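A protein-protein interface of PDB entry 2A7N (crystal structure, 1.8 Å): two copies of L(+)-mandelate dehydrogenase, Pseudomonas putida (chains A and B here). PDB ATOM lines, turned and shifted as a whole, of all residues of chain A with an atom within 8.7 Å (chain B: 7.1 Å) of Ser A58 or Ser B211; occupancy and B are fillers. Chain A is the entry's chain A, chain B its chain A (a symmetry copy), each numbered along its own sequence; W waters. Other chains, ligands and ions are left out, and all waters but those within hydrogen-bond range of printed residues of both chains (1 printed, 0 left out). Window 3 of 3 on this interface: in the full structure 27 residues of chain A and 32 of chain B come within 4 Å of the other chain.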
ATOM      1  N   LEU A  54     -12.558  26.639  27.997  1.00  0.00           N
ATOM      2  CA  LEU A  54     -12.862  27.961  27.475  1.00  0.00           C
ATOM      3  C   LEU A  54     -12.828  28.044  25.957  1.00  0.00           C
ATOM      4  O   LEU A  54     -12.360  29.029  25.382  1.00  0.00           O
ATOM      5  CB  LEU A  54     -11.923  28.995  28.100  1.00  0.00           C
ATOM      6  CG  LEU A  54     -12.264  29.213  29.581  1.00  0.00           C
ATOM      7  CD1 LEU A  54     -11.146  29.956  30.273  1.00  0.00           C
ATOM      8  CD2 LEU A  54     -13.580  29.981  29.698  1.00  0.00           C
ATOM      9  N   VAL A  55     -13.324  26.988  25.316  1.00  0.00           N
ATOM     10  CA  VAL A  55     -13.423  26.936  23.868  1.00  0.00           C
ATOM     11  C   VAL A  55     -14.920  26.984  23.594  1.00  0.00           C
ATOM     12  O   VAL A  55     -15.698  26.293  24.258  1.00  0.00           O
ATOM     13  CB  VAL A  55     -12.853  25.626  23.286  1.00  0.00           C
ATOM     14  CG1 VAL A  55     -13.149  25.549  21.793  1.00  0.00           C
ATOM     15  CG2 VAL A  55     -11.353  25.561  23.521  1.00  0.00           C
ATOM     16  N   ASP A  56     -15.321  27.815  22.639  1.00  0.00           N
ATOM     17  CA  ASP A  56     -16.726  27.949  22.281  1.00  0.00           C
ATOM     18  C   ASP A  56     -17.175  26.675  21.581  1.00  0.00           C
ATOM     19  O   ASP A  56     -16.776  26.408  20.448  1.00  0.00           O
ATOM     20  CB  ASP A  56     -16.912  29.167  21.364  1.00  0.00           C
ATOM     21  CG  ASP A  56     -18.333  29.306  20.837  1.00  0.00           C
ATOM     22  OD1 ASP A  56     -19.229  28.563  21.292  1.00  0.00           O
ATOM     23  OD2 ASP A  56     -18.552  30.171  19.961  1.00  0.00           O
ATOM     24  N   VAL A  57     -17.990  25.880  22.265  1.00  0.00           N
ATOM     25  CA  VAL A  57     -18.492  24.636  21.690  1.00  0.00           C
ATOM     26  C   VAL A  57     -20.010  24.679  21.577  1.00  0.00           C
ATOM     27  O   VAL A  57     -20.677  23.646  21.655  1.00  0.00           O
ATOM     28  CB  VAL A  57     -18.066  23.399  22.538  1.00  0.00           C
ATOM     29  CG1 VAL A  57     -16.545  23.281  22.545  1.00  0.00           C
ATOM     30  CG2 VAL A  57     -18.596  23.515  23.962  1.00  0.00           C
ATOM     31  N   SER A  58     -20.554  25.882  21.386  1.00  0.00           N
ATOM     32  CA  SER A  58     -21.999  26.062  21.258  1.00  0.00           C
ATOM     33  C   SER A  58     -22.490  25.553  19.909  1.00  0.00           C
ATOM     34  O   SER A  58     -23.669  25.243  19.743  1.00  0.00           O
ATOM     35  CB  SER A  58     -22.370  27.542  21.417  1.00  0.00           C
ATOM     36  OG  SER A  58     -21.731  28.333  20.432  1.00  0.00           O
ATOM     37  N   ARG A  59     -21.581  25.483  18.943  1.00  0.00           N
ATOM     38  CA  ARG A  59     -21.901  24.997  17.604  1.00  0.00           C
ATOM     39  C   ARG A  59     -20.924  23.872  17.286  1.00  0.00           C
ATOM     40  O   ARG A  59     -19.747  24.118  17.026  1.00  0.00           O
ATOM     41  CB  ARG A  59     -21.746  26.119  16.571  1.00  0.00           C
ATOM     42  CG  ARG A  59     -22.651  27.321  16.804  1.00  0.00           C
ATOM     43  CD  ARG A  59     -22.394  28.405  15.761  1.00  0.00           C
ATOM     44  NE  ARG A  59     -23.300  29.544  15.903  1.00  0.00           N
ATOM     45  CZ  ARG A  59     -23.341  30.345  16.964  1.00  0.00           C
ATOM     46  NH1 ARG A  59     -22.523  30.142  17.990  1.00  0.00           N
ATOM     47  NH2 ARG A  59     -24.200  31.356  16.998  1.00  0.00           N
ATOM     48  N   ARG A  60     -21.412  22.638  17.316  1.00  0.00           N
ATOM     49  CA  ARG A  60     -20.560  21.486  17.054  1.00  0.00           C
ATOM     50  C   ARG A  60     -20.935  20.776  15.755  1.00  0.00           C
ATOM     51  O   ARG A  60     -22.083  20.826  15.319  1.00  0.00           O
ATOM     52  CB  ARG A  60     -20.642  20.514  18.236  1.00  0.00           C
ATOM     53  CG  ARG A  60     -20.352  21.175  19.583  1.00  0.00           C
ATOM     54  CD  ARG A  60     -20.399  20.184  20.741  1.00  0.00           C
ATOM     55  NE  ARG A  60     -21.749  19.711  21.047  1.00  0.00           N
ATOM     56  CZ  ARG A  60     -22.651  20.394  21.746  1.00  0.00           C
ATOM     57  NH1 ARG A  60     -22.364  21.599  22.225  1.00  0.00           N
ATOM     58  NH2 ARG A  60     -23.843  19.862  21.980  1.00  0.00           N
ATOM     59  N   SER A  61     -19.959  20.113  15.142  1.00  0.00           N
ATOM     60  CA  SER A  61     -20.194  19.395  13.893  1.00  0.00           C
ATOM     61  C   SER A  61     -19.515  18.029  13.894  1.00  0.00           C
ATOM     62  O   SER A  61     -18.318  17.920  14.174  1.00  0.00           O
ATOM     63  CB  SER A  61     -19.684  20.223  12.710  1.00  0.00           C
ATOM     64  OG  SER A  61     -19.724  19.468  11.509  1.00  0.00           O
ATOM     65  N   ASP A 334     -20.998  13.546  20.274  1.00  0.00           N
ATOM     66  CA  ASP A 334     -21.235  14.988  20.340  1.00  0.00           C
ATOM     67  C   ASP A 334     -20.929  15.524  21.740  1.00  0.00           C
ATOM     68  O   ASP A 334     -20.227  16.527  21.905  1.00  0.00           O
ATOM     69  CB  ASP A 334     -22.698  15.277  19.975  1.00  0.00           C
ATOM     70  CG  ASP A 334     -23.057  16.743  20.107  1.00  0.00           C
ATOM     71  OD1 ASP A 334     -22.493  17.572  19.365  1.00  0.00           O
ATOM     72  OD2 ASP A 334     -23.906  17.065  20.961  1.00  0.00           O
ATOM     73  N   ALA A 338     -17.849  18.150  22.967  1.00  0.00           N
ATOM     74  CA  ALA A 338     -18.106  19.361  23.735  1.00  0.00           C
ATOM     75  C   ALA A 338     -17.261  19.388  24.998  1.00  0.00           C
ATOM     76  O   ALA A 338     -16.645  20.403  25.325  1.00  0.00           O
ATOM     77  CB  ALA A 338     -19.588  19.448  24.103  1.00  0.00           C
ATOM     78  N   CYS A 342     -13.434  20.293  21.559  1.00  0.00           N
ATOM     79  CA  CYS A 342     -13.149  20.162  20.130  1.00  0.00           C
ATOM     80  C   CYS A 342     -14.497  20.141  19.410  1.00  0.00           C
ATOM     81  O   CYS A 342     -15.020  19.077  19.079  1.00  0.00           O
ATOM     82  CB  CYS A 342     -12.368  18.866  19.855  1.00  0.00           C
ATOM     83  SG  CYS A 342     -11.699  18.717  18.168  1.00  0.00           S
ATOM     84  N   PRO A 343     -15.072  21.328  19.154  1.00  0.00           N
ATOM     85  CA  PRO A 343     -16.371  21.487  18.485  1.00  0.00           C
ATOM     86  C   PRO A 343     -16.510  20.836  17.118  1.00  0.00           C
ATOM     87  O   PRO A 343     -17.587  20.348  16.769  1.00  0.00           O
ATOM     88  CB  PRO A 343     -16.549  23.005  18.430  1.00  0.00           C
ATOM     89  CG  PRO A 343     -15.146  23.497  18.299  1.00  0.00           C
ATOM     90  CD  PRO A 343     -14.415  22.637  19.323  1.00  0.00           C
ATOM     91  N   ARG B 135     -25.274  35.755  30.105  1.00  0.00           N
ATOM     92  CA  ARG B 135     -24.302  36.779  30.479  1.00  0.00           C
ATOM     93  C   ARG B 135     -24.847  37.822  31.457  1.00  0.00           C
ATOM     94  O   ARG B 135     -24.268  38.045  32.522  1.00  0.00           O
ATOM     95  CB  ARG B 135     -23.761  37.485  29.230  1.00  0.00           C
ATOM     96  CG  ARG B 135     -23.061  36.561  28.230  1.00  0.00           C
ATOM     97  CD  ARG B 135     -21.921  35.782  28.872  1.00  0.00           C
ATOM     98  NE  ARG B 135     -21.332  34.803  27.958  1.00  0.00           N
ATOM     99  CZ  ARG B 135     -20.455  35.090  26.998  1.00  0.00           C
ATOM    100  NH1 ARG B 135     -20.047  36.340  26.815  1.00  0.00           N
ATOM    101  NH2 ARG B 135     -19.987  34.124  26.216  1.00  0.00           N
ATOM    102  N   ALA B 160     -19.862  22.694  30.031  1.00  0.00           N
ATOM    103  CA  ALA B 160     -20.330  23.306  28.791  1.00  0.00           C
ATOM    104  C   ALA B 160     -21.621  22.593  28.409  1.00  0.00           C
ATOM    105  O   ALA B 160     -22.523  23.181  27.817  1.00  0.00           O
ATOM    106  CB  ALA B 160     -19.286  23.140  27.692  1.00  0.00           C
ATOM    107  N   MET B 208     -26.127  25.254  29.918  1.00  0.00           N
ATOM    108  CA  MET B 208     -25.417  26.479  30.279  1.00  0.00           C
ATOM    109  C   MET B 208     -24.735  27.059  29.048  1.00  0.00           C
ATOM    110  O   MET B 208     -24.788  26.472  27.974  1.00  0.00           O
ATOM    111  CB  MET B 208     -24.414  26.219  31.407  1.00  0.00           C
ATOM    112  CG  MET B 208     -25.106  25.950  32.746  1.00  0.00           C
ATOM    113  SD  MET B 208     -23.985  25.606  34.103  1.00  0.00           S
ATOM    114  CE  MET B 208     -24.323  23.870  34.371  1.00  0.00           C
ATOM    115  N   ASP B 209     -24.128  28.229  29.201  1.00  0.00           N
ATOM    116  CA  ASP B 209     -23.471  28.896  28.084  1.00  0.00           C
ATOM    117  C   ASP B 209     -22.231  28.155  27.599  1.00  0.00           C
ATOM    118  O   ASP B 209     -21.156  28.272  28.184  1.00  0.00           O
ATOM    119  CB  ASP B 209     -23.113  30.332  28.473  1.00  0.00           C
ATOM    120  CG  ASP B 209     -22.496  31.107  27.330  1.00  0.00           C
ATOM    121  OD1 ASP B 209     -22.741  30.739  26.160  1.00  0.00           O
ATOM    122  OD2 ASP B 209     -21.776  32.092  27.599  1.00  0.00           O
ATOM    123  N   ALA B 210     -22.383  27.401  26.515  1.00  0.00           N
ATOM    124  CA  ALA B 210     -21.282  26.625  25.959  1.00  0.00           C
ATOM    125  C   ALA B 210     -20.347  27.451  25.081  1.00  0.00           C
ATOM    126  O   ALA B 210     -19.371  26.925  24.543  1.00  0.00           O
ATOM    127  CB  ALA B 210     -21.837  25.453  25.163  1.00  0.00           C
ATOM    128  N   SER B 211     -20.641  28.740  24.932  1.00  0.00           N
ATOM    129  CA  SER B 211     -19.811  29.609  24.104  1.00  0.00           C
ATOM    130  C   SER B 211     -18.792  30.390  24.922  1.00  0.00           C
ATOM    131  O   SER B 211     -17.924  31.058  24.357  1.00  0.00           O
ATOM    132  CB  SER B 211     -20.680  30.602  23.326  1.00  0.00           C
ATOM    133  OG  SER B 211     -21.199  31.610  24.182  1.00  0.00           O
ATOM    134  N   PHE B 212     -18.893  30.310  26.245  1.00  0.00           N
ATOM    135  CA  PHE B 212     -17.974  31.046  27.110  1.00  0.00           C
ATOM    136  C   PHE B 212     -16.530  30.676  26.796  1.00  0.00           C
ATOM    137  O   PHE B 212     -16.094  29.558  27.068  1.00  0.00           O
ATOM    138  CB  PHE B 212     -18.294  30.769  28.581  1.00  0.00           C
ATOM    139  CG  PHE B 212     -17.818  31.844  29.518  1.00  0.00           C
ATOM    140  CD1 PHE B 212     -16.489  31.900  29.923  1.00  0.00           C
ATOM    141  CD2 PHE B 212     -18.698  32.825  29.969  1.00  0.00           C
ATOM    142  CE1 PHE B 212     -16.043  32.911  30.769  1.00  0.00           C
ATOM    143  CE2 PHE B 212     -18.262  33.844  30.816  1.00  0.00           C
ATOM    144  CZ  PHE B 212     -16.930  33.886  31.213  1.00  0.00           C
ATOM    145  N   ASN B 213     -15.796  31.627  26.219  1.00  0.00           N
ATOM    146  CA  ASN B 213     -14.405  31.411  25.836  1.00  0.00           C
ATOM    147  C   ASN B 213     -13.424  32.362  26.516  1.00  0.00           C
ATOM    148  O   ASN B 213     -13.766  33.057  27.470  1.00  0.00           O
ATOM    149  CB  ASN B 213     -14.259  31.548  24.320  1.00  0.00           C
ATOM    150  CG  ASN B 213     -14.791  32.870  23.807  1.00  0.00           C
ATOM    151  OD1 ASN B 213     -14.993  33.809  24.578  1.00  0.00           O
ATOM    152  ND2 ASN B 213     -15.013  32.954  22.500  1.00  0.00           N
ATOM    153  N   TRP B 214     -12.196  32.392  26.007  1.00  0.00           N
ATOM    154  CA  TRP B 214     -11.157  33.242  26.574  1.00  0.00           C
ATOM    155  C   TRP B 214     -11.560  34.709  26.587  1.00  0.00           C
ATOM    156  O   TRP B 214     -11.321  35.411  27.567  1.00  0.00           O
ATOM    157  CB  TRP B 214      -9.844  33.055  25.811  1.00  0.00           C
ATOM    158  CG  TRP B 214      -9.331  31.649  25.887  1.00  0.00           C
ATOM    159  CD1 TRP B 214      -9.309  30.726  24.882  1.00  0.00           C
ATOM    160  CD2 TRP B 214      -8.820  30.987  27.049  1.00  0.00           C
ATOM    161  NE1 TRP B 214      -8.820  29.527  25.345  1.00  0.00           N
ATOM    162  CE2 TRP B 214      -8.510  29.660  26.677  1.00  0.00           C
ATOM    163  CE3 TRP B 214      -8.594  31.383  28.375  1.00  0.00           C
ATOM    164  CZ2 TRP B 214      -7.990  28.726  27.577  1.00  0.00           C
ATOM    165  CZ3 TRP B 214      -8.076  30.455  29.272  1.00  0.00           C
ATOM    166  CH2 TRP B 214      -7.780  29.142  28.868  1.00  0.00           C
ATOM    167  N   ALA B 216     -14.524  35.875  26.776  1.00  0.00           N
ATOM    168  CA  ALA B 216     -15.535  36.015  27.819  1.00  0.00           C
ATOM    169  C   ALA B 216     -14.871  36.070  29.194  1.00  0.00           C
ATOM    170  O   ALA B 216     -15.367  36.737  30.107  1.00  0.00           O
ATOM    171  CB  ALA B 216     -16.528  34.850  27.748  1.00  0.00           C
HETATM  172  O   HOH W   1     -16.653  26.842  26.942  1.00  0.00           O
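Among the printed residues, pairs that only touch across the chains: Leu A54 with Phe B212, Leu A54 with Asn B213, Val A55 with Ala B210, Asp A56 with Ala B210, Asp A56 with Ser B211, Val A57 with Ala B160, Ser A58 with Ala B210 and Ser A58 with Ser B211.
The side-chain carboxylate (OD1) of Asp A56 sits at hydrogen-bond distance from the side-chain hydroxyl (OG) of Ser A58 (2.7 Å).
NH1 of Arg A60 sits at hydrogen-bond distance from O of Val A57, 2.7 Å away.
The side-chain hydroxyl (OG) of Ser A58 lies within hydrogen-bond range of the guanidinium group (NH1) of Arg A59 (3.1 Å).
The guanidinium group (NH2) of Arg B135 lies within hydrogen-bond range of the side-chain hydroxyl (OG) of Ser B211.
The side-chain carboxylate (OD1) of Asp B209 sits at hydrogen-bond distance from the side-chain hydroxyl (OG) of Ser B211, 2.7 Å away.
The side-chain amide oxygen (OD1) of Asn B213 lies within hydrogen-bond range of the backbone NH (N) of Ala B216, at 3.1 Å.
No position is printed for both chains.
Of the printed residues of chain B, Val A55 touches Ala B210 (3.7 Å).
Printed residues of chain B within 4 Å of Asp A56: Ala B210 (3.6 Å) and Ser B211 (3.1 Å).
Arg B135 touches none of the printed residues of chain A.
Of the printed residues of chain A, Ala B160 touches Val A57.
Ala B210 touches just these residues of chain A: Val A55 (3.7 Å), Asp A56 (3.6 Å), Val A57 (2.9 Å) and Ser A58 (3.5 Å).
Of the printed residues of chain A, Ser B211 touches Asp A56 (3.1 Å) and Ser A58 (3.8 Å).
The nearest residue of chain B that does not touch Ser A58 is Asp B209 (5.7 Å).
The nearest residue of chain A that does not touch Ser B211 is Val A57 (4.5 Å).
The nearest printed residue of chain B that does not touch Asp A56 is Asn B213 (4.2 Å).
Water W1 bridges O of Phe B212 (2.8 Å) and O of Val A55 (2.9 Å).
Of the 12 printed residues of chain A, 5 touch a printed residue of chain B.
Hydrophobic or aromatic side chains of chain A within 4 Å of the printed part of chain B: Leu A54 and Val A57.
Of the 10 printed residues of chain B, 6 touch a printed residue of chain A.
Among the printed residues, 10 pairs touch across the chains.
Among the printed residues, no Asp or Glu carboxylate lies within 4 Å of a Lys or Arg side-chain nitrogen of the other chain.
The backbone carbonyl oxygen of Leu A54 sits at hydrogen-bond distance from the backbone NH of Trp B214.
N of Val A57 is in hydrogen-bond range of O of Ala B210, 2.9 Å away.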
